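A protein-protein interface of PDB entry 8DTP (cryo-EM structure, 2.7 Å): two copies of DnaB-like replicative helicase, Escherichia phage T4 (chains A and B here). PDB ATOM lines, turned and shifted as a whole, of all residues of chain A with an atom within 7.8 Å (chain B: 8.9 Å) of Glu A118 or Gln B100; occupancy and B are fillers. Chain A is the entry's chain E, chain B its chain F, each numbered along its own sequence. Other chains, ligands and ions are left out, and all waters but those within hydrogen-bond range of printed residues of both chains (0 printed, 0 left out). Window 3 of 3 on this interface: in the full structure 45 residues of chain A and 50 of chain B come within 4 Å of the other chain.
Among the printed residues, merely in contact across the chains: Ile A111 with Thr B107 (3.8 Å), Glu A118 with Gln B100 (3.9 Å) and Val A131 with Leu B142 (3.4 Å).
Of the printed residues of chain B, Ile A111 touches Thr B107 (3.8 Å).
Asn A116 touches none of the printed residues of chain B.
No residue of chain B comes within 4 Å of Ala A117.
Glu A118 touches just one residue of chain B: Gln B100 (3.9 Å).
Of the printed residues of chain B, Val A131 touches Leu B142.
Gln B100 touches one residue of chain A.
Printed residues of chain A within 4 Å of Met B103: Gln A114 (3.5 Å).
Printed residues of chain A within 4 Å of Thr B107: Ile A111 and Gln A114.
Of the printed residues of chain A, Leu B142 touches Val A131.
The nearest residue of chain B that does not touch Glu A118 is Phe B104 (5.9 Å).
The nearest residue of chain A that does not touch Gln B100 is Ala A117 (5.7 Å).
The backbone carbonyl oxygen (O) of Ile A111 lies within hydrogen-bond range of the side-chain hydroxyl (OG1) of Thr A115, at 3.0 Å.
The side-chain hydroxyl of Thr B107 sits at hydrogen-bond distance from the backbone carbonyl oxygen of Met B103, 2.9 Å away.
No position is printed for both chains.
Of the 5 pairs that touch across the chains among the printed residues, none has its exchanged pair printed and touching as well.
Printed residues of chain A that touch a printed residue of chain B: Ile A111, Gln A114, Glu A118 and Val A131.
Hydrophobic or aromatic side chains of chain A within 4 Å of the printed part of chain B: Ile A111 and Val A131.
Hydrophobic or aromatic side chains of chain B that line the printed part of chain A: Met B103 and Leu B142.
Along chain B the printed residues that touch a printed residue of chain A span positions 100 to 142.
Among the printed residues, no Asp or Glu carboxylate lies within 4 Å of a Lys or Arg side-chain nitrogen of the other chain.
The side-chain amide nitrogen (NE2) of Gln A114 sits at hydrogen-bond distance from the backbone carbonyl oxygen (O) of Met B103 (3.5 Å).
NE2 of Gln A114 lies within hydrogen-bond range of OG1 of Thr B107 (2.8 Å).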
ATOM      1  N   ILE A 111     -16.272 -10.191  27.726  1.00  0.00           N
ATOM      2  CA  ILE A 111     -16.533 -10.379  26.300  1.00  0.00           C
ATOM      3  C   ILE A 111     -16.656 -11.863  25.976  1.00  0.00           C
ATOM      4  O   ILE A 111     -17.537 -12.276  25.210  1.00  0.00           O
ATOM      5  CB  ILE A 111     -15.441  -9.695  25.456  1.00  0.00           C
ATOM      6  CG1 ILE A 111     -15.605  -8.176  25.510  1.00  0.00           C
ATOM      7  CG2 ILE A 111     -15.489 -10.180  24.020  1.00  0.00           C
ATOM      8  CD1 ILE A 111     -14.630  -7.425  24.640  1.00  0.00           C
ATOM      9  N   GLU A 112     -15.784 -12.689  26.559  1.00  0.00           N
ATOM     10  CA  GLU A 112     -15.884 -14.131  26.355  1.00  0.00           C
ATOM     11  C   GLU A 112     -17.180 -14.682  26.934  1.00  0.00           C
ATOM     12  O   GLU A 112     -17.799 -15.575  26.344  1.00  0.00           O
ATOM     13  CB  GLU A 112     -14.678 -14.840  26.971  1.00  0.00           C
ATOM     14  CG  GLU A 112     -13.366 -14.566  26.261  1.00  0.00           C
ATOM     15  CD  GLU A 112     -12.201 -15.302  26.890  1.00  0.00           C
ATOM     16  OE1 GLU A 112     -12.411 -15.989  27.912  1.00  0.00           O
ATOM     17  OE2 GLU A 112     -11.074 -15.195  26.361  1.00  0.00           O
ATOM     18  N   ILE A 113     -17.602 -14.172  28.093  1.00  0.00           N
ATOM     19  CA  ILE A 113     -18.865 -14.609  28.688  1.00  0.00           C
ATOM     20  C   ILE A 113     -20.030 -14.279  27.762  1.00  0.00           C
ATOM     21  O   ILE A 113     -20.917 -15.109  27.530  1.00  0.00           O
ATOM     22  CB  ILE A 113     -19.053 -13.971  30.076  1.00  0.00           C
ATOM     23  CG1 ILE A 113     -18.082 -14.583  31.085  1.00  0.00           C
ATOM     24  CG2 ILE A 113     -20.487 -14.133  30.552  1.00  0.00           C
ATOM     25  CD1 ILE A 113     -18.216 -14.013  32.477  1.00  0.00           C
ATOM     26  N   GLN A 114     -20.042 -13.060  27.217  1.00  0.00           N
ATOM     27  CA  GLN A 114     -21.109 -12.670  26.301  1.00  0.00           C
ATOM     28  C   GLN A 114     -21.102 -13.528  25.042  1.00  0.00           C
ATOM     29  O   GLN A 114     -22.163 -13.941  24.560  1.00  0.00           O
ATOM     30  CB  GLN A 114     -20.976 -11.193  25.935  1.00  0.00           C
ATOM     31  CG  GLN A 114     -21.275 -10.240  27.073  1.00  0.00           C
ATOM     32  CD  GLN A 114     -21.106  -8.793  26.667  1.00  0.00           C
ATOM     33  OE1 GLN A 114     -20.606  -8.496  25.583  1.00  0.00           O
ATOM     34  NE2 GLN A 114     -21.525  -7.881  27.535  1.00  0.00           N
ATOM     35  N   THR A 115     -19.918 -13.802  24.491  1.00  0.00           N
ATOM     36  CA  THR A 115     -19.835 -14.637  23.296  1.00  0.00           C
ATOM     37  C   THR A 115     -20.322 -16.054  23.577  1.00  0.00           C
ATOM     38  O   THR A 115     -21.025 -16.652  22.755  1.00  0.00           O
ATOM     39  CB  THR A 115     -18.401 -14.654  22.766  1.00  0.00           C
ATOM     40  OG1 THR A 115     -17.996 -13.318  22.442  1.00  0.00           O
ATOM     41  CG2 THR A 115     -18.299 -15.519  21.522  1.00  0.00           C
ATOM     42  N   ASN A 116     -19.965 -16.605  24.739  1.00  0.00           N
ATOM     43  CA  ASN A 116     -20.411 -17.946  25.098  1.00  0.00           C
ATOM     44  C   ASN A 116     -21.910 -17.992  25.363  1.00  0.00           C
ATOM     45  O   ASN A 116     -22.549 -19.023  25.124  1.00  0.00           O
ATOM     46  CB  ASN A 116     -19.638 -18.442  26.320  1.00  0.00           C
ATOM     47  CG  ASN A 116     -20.179 -19.746  26.865  1.00  0.00           C
ATOM     48  OD1 ASN A 116     -19.870 -20.822  26.356  1.00  0.00           O
ATOM     49  ND2 ASN A 116     -20.989 -19.656  27.914  1.00  0.00           N
ATOM     50  N   ALA A 117     -22.486 -16.894  25.859  1.00  0.00           N
ATOM     51  CA  ALA A 117     -23.917 -16.875  26.146  1.00  0.00           C
ATOM     52  C   ALA A 117     -24.743 -17.033  24.875  1.00  0.00           C
ATOM     53  O   ALA A 117     -25.786 -17.696  24.883  1.00  0.00           O
ATOM     54  CB  ALA A 117     -24.289 -15.581  26.869  1.00  0.00           C
ATOM     55  N   GLU A 118     -24.294 -16.431  23.772  1.00  0.00           N
ATOM     56  CA  GLU A 118     -25.040 -16.507  22.522  1.00  0.00           C
ATOM     57  C   GLU A 118     -24.999 -17.897  21.900  1.00  0.00           C
ATOM     58  O   GLU A 118     -25.809 -18.187  21.012  1.00  0.00           O
ATOM     59  CB  GLU A 118     -24.503 -15.481  21.525  1.00  0.00           C
ATOM     60  CG  GLU A 118     -24.569 -14.047  22.017  1.00  0.00           C
ATOM     61  CD  GLU A 118     -24.032 -13.059  21.001  1.00  0.00           C
ATOM     62  OE1 GLU A 118     -23.658 -13.492  19.890  1.00  0.00           O
ATOM     63  OE2 GLU A 118     -23.980 -11.850  21.314  1.00  0.00           O
ATOM     64  N   LEU A 119     -24.082 -18.754  22.335  1.00  0.00           N
ATOM     65  CA  LEU A 119     -23.989 -20.092  21.779  1.00  0.00           C
ATOM     66  C   LEU A 119     -25.184 -20.939  22.220  1.00  0.00           C
ATOM     67  O   LEU A 119     -25.792 -20.674  23.260  1.00  0.00           O
ATOM     68  CB  LEU A 119     -22.690 -20.763  22.214  1.00  0.00           C
ATOM     69  CG  LEU A 119     -21.390 -20.113  21.740  1.00  0.00           C
ATOM     70  CD1 LEU A 119     -20.187 -20.885  22.258  1.00  0.00           C
ATOM     71  CD2 LEU A 119     -21.357 -20.021  20.223  1.00  0.00           C
ATOM     72  N   PRO A 120     -25.548 -21.951  21.434  1.00  0.00           N
ATOM     73  CA  PRO A 120     -26.612 -22.853  21.861  1.00  0.00           C
ATOM     74  C   PRO A 120     -26.215 -23.583  23.127  1.00  0.00           C
ATOM     75  O   PRO A 120     -25.017 -23.804  23.389  1.00  0.00           O
ATOM     76  CB  PRO A 120     -26.753 -23.817  20.674  1.00  0.00           C
ATOM     77  CG  PRO A 120     -26.232 -23.053  19.507  1.00  0.00           C
ATOM     78  CD  PRO A 120     -25.116 -22.217  20.051  1.00  0.00           C
ATOM     79  N   PRO A 121     -27.190 -23.969  23.955  1.00  0.00           N
ATOM     80  CA  PRO A 121     -26.854 -24.602  25.243  1.00  0.00           C
ATOM     81  C   PRO A 121     -26.018 -25.863  25.109  1.00  0.00           C
ATOM     82  O   PRO A 121     -25.193 -26.141  25.988  1.00  0.00           O
ATOM     83  CB  PRO A 121     -28.230 -24.900  25.854  1.00  0.00           C
ATOM     84  CG  PRO A 121     -29.156 -23.931  25.195  1.00  0.00           C
ATOM     85  CD  PRO A 121     -28.640 -23.771  23.796  1.00  0.00           C
ATOM     86  N   ARG A 124     -22.369 -24.514  24.325  1.00  0.00           N
ATOM     87  CA  ARG A 124     -21.747 -23.602  25.276  1.00  0.00           C
ATOM     88  C   ARG A 124     -21.028 -24.362  26.386  1.00  0.00           C
ATOM     89  O   ARG A 124     -21.409 -25.474  26.765  1.00  0.00           O
ATOM     90  CB  ARG A 124     -22.788 -22.660  25.878  1.00  0.00           C
ATOM     91  CG  ARG A 124     -23.811 -23.334  26.768  1.00  0.00           C
ATOM     92  CD  ARG A 124     -24.743 -22.310  27.388  1.00  0.00           C
ATOM     93  NE  ARG A 124     -25.341 -21.443  26.381  1.00  0.00           N
ATOM     94  CZ  ARG A 124     -26.228 -20.493  26.643  1.00  0.00           C
ATOM     95  NH1 ARG A 124     -26.646 -20.259  27.876  1.00  0.00           N
ATOM     96  NH2 ARG A 124     -26.707 -19.760  25.642  1.00  0.00           N
ATOM     97  N   VAL A 131     -24.156 -14.397  32.337  1.00  0.00           N
ATOM     98  CA  VAL A 131     -24.044 -12.955  32.138  1.00  0.00           C
ATOM     99  C   VAL A 131     -24.261 -12.205  33.445  1.00  0.00           C
ATOM    100  O   VAL A 131     -23.749 -11.093  33.623  1.00  0.00           O
ATOM    101  CB  VAL A 131     -25.026 -12.489  31.049  1.00  0.00           C
ATOM    102  CG1 VAL A 131     -24.617 -13.047  29.698  1.00  0.00           C
ATOM    103  CG2 VAL A 131     -26.443 -12.912  31.397  1.00  0.00           C
ATOM    104  N   MET B   1     -32.403 -10.658  14.179  1.00  0.00           N
ATOM    105  CA  MET B   1     -33.718 -10.778  13.562  1.00  0.00           C
ATOM    106  C   MET B   1     -34.415  -9.424  13.477  1.00  0.00           C
ATOM    107  O   MET B   1     -35.594  -9.300  13.807  1.00  0.00           O
ATOM    108  CB  MET B   1     -34.586 -11.768  14.340  1.00  0.00           C
ATOM    109  CG  MET B   1     -34.651 -11.502  15.832  1.00  0.00           C
ATOM    110  SD  MET B   1     -35.965 -12.435  16.636  1.00  0.00           S
ATOM    111  CE  MET B   1     -35.529 -14.105  16.162  1.00  0.00           C
ATOM    112  N   GLU B  26     -31.192   2.492  19.671  1.00  0.00           N
ATOM    113  CA  GLU B  26     -29.838   1.992  19.877  1.00  0.00           C
ATOM    114  C   GLU B  26     -29.731   0.481  19.724  1.00  0.00           C
ATOM    115  O   GLU B  26     -28.612  -0.042  19.698  1.00  0.00           O
ATOM    116  CB  GLU B  26     -29.332   2.410  21.257  1.00  0.00           C
ATOM    117  CG  GLU B  26     -29.272   3.916  21.471  1.00  0.00           C
ATOM    118  CD  GLU B  26     -28.239   4.598  20.594  1.00  0.00           C
ATOM    119  OE1 GLU B  26     -27.281   3.923  20.160  1.00  0.00           O
ATOM    120  OE2 GLU B  26     -28.384   5.811  20.336  1.00  0.00           O
ATOM    121  N   TYR B  27     -30.853  -0.227  19.622  1.00  0.00           N
ATOM    122  CA  TYR B  27     -30.854  -1.677  19.495  1.00  0.00           C
ATOM    123  C   TYR B  27     -30.696  -2.149  18.056  1.00  0.00           C
ATOM    124  O   TYR B  27     -30.704  -3.360  17.815  1.00  0.00           O
ATOM    125  CB  TYR B  27     -32.144  -2.258  20.082  1.00  0.00           C
ATOM    126  CG  TYR B  27     -32.352  -1.942  21.545  1.00  0.00           C
ATOM    127  CD1 TYR B  27     -31.276  -1.821  22.408  1.00  0.00           C
ATOM    128  CD2 TYR B  27     -33.625  -1.761  22.061  1.00  0.00           C
ATOM    129  CE1 TYR B  27     -31.461  -1.531  23.743  1.00  0.00           C
ATOM    130  CE2 TYR B  27     -33.819  -1.469  23.395  1.00  0.00           C
ATOM    131  CZ  TYR B  27     -32.735  -1.356  24.231  1.00  0.00           C
ATOM    132  OH  TYR B  27     -32.925  -1.066  25.561  1.00  0.00           O
ATOM    133  N   GLU B  29     -28.639  -1.840  14.139  1.00  0.00           N
ATOM    134  CA  GLU B  29     -27.404  -1.461  13.475  1.00  0.00           C
ATOM    135  C   GLU B  29     -27.600  -0.181  12.667  1.00  0.00           C
ATOM    136  O   GLU B  29     -28.708   0.153  12.237  1.00  0.00           O
ATOM    137  CB  GLU B  29     -26.912  -2.591  12.571  1.00  0.00           C
ATOM    138  CG  GLU B  29     -26.476  -3.839  13.322  1.00  0.00           C
ATOM    139  CD  GLU B  29     -25.226  -3.617  14.152  1.00  0.00           C
ATOM    140  OE1 GLU B  29     -24.454  -2.688  13.836  1.00  0.00           O
ATOM    141  OE2 GLU B  29     -25.016  -4.371  15.125  1.00  0.00           O
ATOM    142  N   LYS B  92     -40.355 -13.589  23.225  1.00  0.00           N
ATOM    143  CA  LYS B  92     -39.139 -14.004  23.916  1.00  0.00           C
ATOM    144  C   LYS B  92     -37.908 -13.820  23.036  1.00  0.00           C
ATOM    145  O   LYS B  92     -36.844 -13.427  23.528  1.00  0.00           O
ATOM    146  CB  LYS B  92     -39.264 -15.452  24.392  1.00  0.00           C
ATOM    147  CG  LYS B  92     -39.556 -16.464  23.302  1.00  0.00           C
ATOM    148  CD  LYS B  92     -39.744 -17.856  23.880  1.00  0.00           C
ATOM    149  CE  LYS B  92     -38.494 -18.327  24.601  1.00  0.00           C
ATOM    150  NZ  LYS B  92     -37.317 -18.372  23.692  1.00  0.00           N
ATOM    151  N   GLU B  93     -38.027 -14.091  21.732  1.00  0.00           N
ATOM    152  CA  GLU B  93     -36.895 -13.864  20.839  1.00  0.00           C
ATOM    153  C   GLU B  93     -36.541 -12.384  20.758  1.00  0.00           C
ATOM    154  O   GLU B  93     -35.358 -12.020  20.750  1.00  0.00           O
ATOM    155  CB  GLU B  93     -37.200 -14.422  19.450  1.00  0.00           C
ATOM    156  CG  GLU B  93     -37.036 -15.925  19.346  1.00  0.00           C
ATOM    157  CD  GLU B  93     -35.588 -16.364  19.439  1.00  0.00           C
ATOM    158  OE1 GLU B  93     -34.693 -15.535  19.174  1.00  0.00           O
ATOM    159  OE2 GLU B  93     -35.346 -17.541  19.781  1.00  0.00           O
ATOM    160  N   THR B  94     -37.552 -11.516  20.696  1.00  0.00           N
ATOM    161  CA  THR B  94     -37.296 -10.080  20.688  1.00  0.00           C
ATOM    162  C   THR B  94     -36.643  -9.637  21.989  1.00  0.00           C
ATOM    163  O   THR B  94     -35.736  -8.797  21.982  1.00  0.00           O
ATOM    164  CB  THR B  94     -38.598  -9.314  20.457  1.00  0.00           C
ATOM    165  OG1 THR B  94     -39.246  -9.818  19.282  1.00  0.00           O
ATOM    166  CG2 THR B  94     -38.318  -7.832  20.270  1.00  0.00           C
ATOM    167  N   GLU B  95     -37.095 -10.187  23.118  1.00  0.00           N
ATOM    168  CA  GLU B  95     -36.484  -9.845  24.397  1.00  0.00           C
ATOM    169  C   GLU B  95     -35.022 -10.274  24.438  1.00  0.00           C
ATOM    170  O   GLU B  95     -34.158  -9.524  24.907  1.00  0.00           O
ATOM    171  CB  GLU B  95     -37.271 -10.486  25.539  1.00  0.00           C
ATOM    172  CG  GLU B  95     -36.987  -9.881  26.900  1.00  0.00           C
ATOM    173  CD  GLU B  95     -37.890 -10.438  27.983  1.00  0.00           C
ATOM    174  OE1 GLU B  95     -38.573 -11.452  27.728  1.00  0.00           O
ATOM    175  OE2 GLU B  95     -37.918  -9.860  29.090  1.00  0.00           O
ATOM    176  N   LYS B  96     -34.726 -11.477  23.938  1.00  0.00           N
ATOM    177  CA  LYS B  96     -33.343 -11.939  23.875  1.00  0.00           C
ATOM    178  C   LYS B  96     -32.497 -11.027  22.996  1.00  0.00           C
ATOM    179  O   LYS B  96     -31.368 -10.674  23.359  1.00  0.00           O
ATOM    180  CB  LYS B  96     -33.289 -13.373  23.352  1.00  0.00           C
ATOM    181  CG  LYS B  96     -33.870 -14.412  24.292  1.00  0.00           C
ATOM    182  CD  LYS B  96     -33.928 -15.797  23.650  1.00  0.00           C
ATOM    183  CE  LYS B  96     -32.543 -16.387  23.410  1.00  0.00           C
ATOM    184  NZ  LYS B  96     -31.943 -15.976  22.109  1.00  0.00           N
ATOM    185  N   TYR B  97     -33.026 -10.643  21.834  1.00  0.00           N
ATOM    186  CA  TYR B  97     -32.281  -9.773  20.929  1.00  0.00           C
ATOM    187  C   TYR B  97     -32.012  -8.418  21.569  1.00  0.00           C
ATOM    188  O   TYR B  97     -30.905  -7.876  21.454  1.00  0.00           O
ATOM    189  CB  TYR B  97     -33.048  -9.615  19.618  1.00  0.00           C
ATOM    190  CG  TYR B  97     -32.334  -8.803  18.566  1.00  0.00           C
ATOM    191  CD1 TYR B  97     -31.382  -9.382  17.742  1.00  0.00           C
ATOM    192  CD2 TYR B  97     -32.622  -7.458  18.387  1.00  0.00           C
ATOM    193  CE1 TYR B  97     -30.730  -8.643  16.775  1.00  0.00           C
ATOM    194  CE2 TYR B  97     -31.975  -6.713  17.424  1.00  0.00           C
ATOM    195  CZ  TYR B  97     -31.030  -7.310  16.621  1.00  0.00           C
ATOM    196  OH  TYR B  97     -30.384  -6.570  15.660  1.00  0.00           O
ATOM    197  N   VAL B  98     -33.010  -7.858  22.255  1.00  0.00           N
ATOM    198  CA  VAL B  98     -32.838  -6.564  22.903  1.00  0.00           C
ATOM    199  C   VAL B  98     -31.809  -6.654  24.022  1.00  0.00           C
ATOM    200  O   VAL B  98     -30.974  -5.756  24.189  1.00  0.00           O
ATOM    201  CB  VAL B  98     -34.196  -6.043  23.411  1.00  0.00           C
ATOM    202  CG1 VAL B  98     -34.004  -4.825  24.289  1.00  0.00           C
ATOM    203  CG2 VAL B  98     -35.098  -5.705  22.238  1.00  0.00           C
ATOM    204  N   GLN B  99     -31.844  -7.736  24.806  1.00  0.00           N
ATOM    205  CA  GLN B  99     -30.853  -7.914  25.863  1.00  0.00           C
ATOM    206  C   GLN B  99     -29.445  -8.037  25.289  1.00  0.00           C
ATOM    207  O   GLN B  99     -28.495  -7.447  25.819  1.00  0.00           O
ATOM    208  CB  GLN B  99     -31.207  -9.137  26.706  1.00  0.00           C
ATOM    209  CG  GLN B  99     -32.466  -8.960  27.536  1.00  0.00           C
ATOM    210  CD  GLN B  99     -33.010 -10.270  28.067  1.00  0.00           C
ATOM    211  OE1 GLN B  99     -32.518 -11.344  27.726  1.00  0.00           O
ATOM    212  NE2 GLN B  99     -34.033 -10.187  28.907  1.00  0.00           N
ATOM    213  N   GLN B 100     -29.291  -8.799  24.202  1.00  0.00           N
ATOM    214  CA  GLN B 100     -27.983  -8.926  23.569  1.00  0.00           C
ATOM    215  C   GLN B 100     -27.485  -7.582  23.050  1.00  0.00           C
ATOM    216  O   GLN B 100     -26.304  -7.248  23.206  1.00  0.00           O
ATOM    217  CB  GLN B 100     -28.040  -9.943  22.431  1.00  0.00           C
ATOM    218  CG  GLN B 100     -28.258 -11.372  22.886  1.00  0.00           C
ATOM    219  CD  GLN B 100     -28.195 -12.357  21.739  1.00  0.00           C
ATOM    220  OE1 GLN B 100     -27.864 -11.993  20.610  1.00  0.00           O
ATOM    221  NE2 GLN B 100     -28.514 -13.615  22.021  1.00  0.00           N
ATOM    222  N   ARG B 101     -28.367  -6.803  22.423  1.00  0.00           N
ATOM    223  CA  ARG B 101     -27.961  -5.495  21.919  1.00  0.00           C
ATOM    224  C   ARG B 101     -27.570  -4.561  23.057  1.00  0.00           C
ATOM    225  O   ARG B 101     -26.602  -3.801  22.941  1.00  0.00           O
ATOM    226  CB  ARG B 101     -29.080  -4.881  21.080  1.00  0.00           C
ATOM    227  CG  ARG B 101     -29.379  -5.644  19.803  1.00  0.00           C
ATOM    228  CD  ARG B 101     -28.108  -5.905  19.018  1.00  0.00           C
ATOM    229  NE  ARG B 101     -27.396  -4.671  18.715  1.00  0.00           N
ATOM    230  CZ  ARG B 101     -26.225  -4.614  18.097  1.00  0.00           C
ATOM    231  NH1 ARG B 101     -25.599  -5.711  17.704  1.00  0.00           N
ATOM    232  NH2 ARG B 101     -25.668  -3.429  17.869  1.00  0.00           N
ATOM    233  N   ALA B 102     -28.313  -4.602  24.165  1.00  0.00           N
ATOM    234  CA  ALA B 102     -27.967  -3.777  25.316  1.00  0.00           C
ATOM    235  C   ALA B 102     -26.606  -4.162  25.879  1.00  0.00           C
ATOM    236  O   ALA B 102     -25.797  -3.290  26.221  1.00  0.00           O
ATOM    237  CB  ALA B 102     -29.049  -3.892  26.389  1.00  0.00           C
ATOM    238  N   MET B 103     -26.332  -5.465  25.977  1.00  0.00           N
ATOM    239  CA  MET B 103     -25.025  -5.910  26.451  1.00  0.00           C
ATOM    240  C   MET B 103     -23.912  -5.466  25.510  1.00  0.00           C
ATOM    241  O   MET B 103     -22.838  -5.050  25.960  1.00  0.00           O
ATOM    242  CB  MET B 103     -25.016  -7.428  26.616  1.00  0.00           C
ATOM    243  CG  MET B 103     -25.828  -7.941  27.794  1.00  0.00           C
ATOM    244  SD  MET B 103     -24.818  -8.374  29.225  1.00  0.00           S
ATOM    245  CE  MET B 103     -24.376  -6.761  29.862  1.00  0.00           C
ATOM    246  N   PHE B 104     -24.148  -5.558  24.199  1.00  0.00           N
ATOM    247  CA  PHE B 104     -23.148  -5.121  23.230  1.00  0.00           C
ATOM    248  C   PHE B 104     -22.863  -3.630  23.369  1.00  0.00           C
ATOM    249  O   PHE B 104     -21.698  -3.203  23.359  1.00  0.00           O
ATOM    250  CB  PHE B 104     -23.627  -5.448  21.816  1.00  0.00           C
ATOM    251  CG  PHE B 104     -22.566  -5.309  20.764  1.00  0.00           C
ATOM    252  CD1 PHE B 104     -22.322  -4.087  20.161  1.00  0.00           C
ATOM    253  CD2 PHE B 104     -21.823  -6.405  20.366  1.00  0.00           C
ATOM    254  CE1 PHE B 104     -21.351  -3.959  19.192  1.00  0.00           C
ATOM    255  CE2 PHE B 104     -20.850  -6.283  19.396  1.00  0.00           C
ATOM    256  CZ  PHE B 104     -20.613  -5.060  18.808  1.00  0.00           C
ATOM    257  N   ASN B 105     -23.916  -2.822  23.504  1.00  0.00           N
ATOM    258  CA  ASN B 105     -23.733  -1.385  23.665  1.00  0.00           C
ATOM    259  C   ASN B 105     -22.987  -1.067  24.955  1.00  0.00           C
ATOM    260  O   ASN B 105     -22.113  -0.192  24.974  1.00  0.00           O
ATOM    261  CB  ASN B 105     -25.085  -0.673  23.637  1.00  0.00           C
ATOM    262  CG  ASN B 105     -25.821  -0.872  22.328  1.00  0.00           C
ATOM    263  OD1 ASN B 105     -25.224  -1.233  21.316  1.00  0.00           O
ATOM    264  ND2 ASN B 105     -27.125  -0.632  22.342  1.00  0.00           N
ATOM    265  N   ALA B 106     -23.316  -1.768  26.042  1.00  0.00           N
ATOM    266  CA  ALA B 106     -22.615  -1.548  27.303  1.00  0.00           C
ATOM    267  C   ALA B 106     -21.140  -1.911  27.190  1.00  0.00           C
ATOM    268  O   ALA B 106     -20.277  -1.202  27.723  1.00  0.00           O
ATOM    269  CB  ALA B 106     -23.281  -2.351  28.420  1.00  0.00           C
ATOM    270  N   THR B 107     -20.830  -3.018  26.511  1.00  0.00           N
ATOM    271  CA  THR B 107     -19.435  -3.408  26.328  1.00  0.00           C
ATOM    272  C   THR B 107     -18.670  -2.362  25.527  1.00  0.00           C
ATOM    273  O   THR B 107     -17.550  -1.980  25.894  1.00  0.00           O
ATOM    274  CB  THR B 107     -19.359  -4.770  25.641  1.00  0.00           C
ATOM    275  OG1 THR B 107     -20.054  -5.742  26.430  1.00  0.00           O
ATOM    276  CG2 THR B 107     -17.914  -5.205  25.474  1.00  0.00           C
ATOM    277  N   ALA B 141     -27.574  -2.720  31.862  1.00  0.00           N
ATOM    278  CA  ALA B 141     -27.856  -3.483  30.649  1.00  0.00           C
ATOM    279  C   ALA B 141     -28.529  -4.812  30.968  1.00  0.00           C
ATOM    280  O   ALA B 141     -29.434  -5.245  30.245  1.00  0.00           O
ATOM    281  CB  ALA B 141     -26.565  -3.710  29.864  1.00  0.00           C
ATOM    282  N   LEU B 142     -28.100  -5.477  32.041  1.00  0.00           N
ATOM    283  CA  LEU B 142     -28.692  -6.756  32.415  1.00  0.00           C
ATOM    284  C   LEU B 142     -30.125  -6.615  32.910  1.00  0.00           C
ATOM    285  O   LEU B 142     -30.843  -7.617  32.979  1.00  0.00           O
ATOM    286  CB  LEU B 142     -27.842  -7.434  33.490  1.00  0.00           C
ATOM    287  CG  LEU B 142     -26.480  -7.974  33.056  1.00  0.00           C
ATOM    288  CD1 LEU B 142     -25.629  -8.303  34.269  1.00  0.00           C
ATOM    289  CD2 LEU B 142     -26.657  -9.203  32.184  1.00  0.00           C
ATOM    290  N   ILE B 144     -32.533  -4.994  31.404  1.00  0.00           N
ATOM    291  CA  ILE B 144     -33.477  -4.773  30.316  1.00  0.00           C
ATOM    292  C   ILE B 144     -34.402  -5.975  30.196  1.00  0.00           C
ATOM    293  O   ILE B 144     -33.952  -7.127  30.135  1.00  0.00           O
ATOM    294  CB  ILE B 144     -32.731  -4.497  29.001  1.00  0.00           C
ATOM    295  CG1 ILE B 144     -32.543  -2.993  28.788  1.00  0.00           C
ATOM    296  CG2 ILE B 144     -33.475  -5.089  27.820  1.00  0.00           C
ATOM    297  CD1 ILE B 144     -31.633  -2.329  29.789  1.00  0.00           C
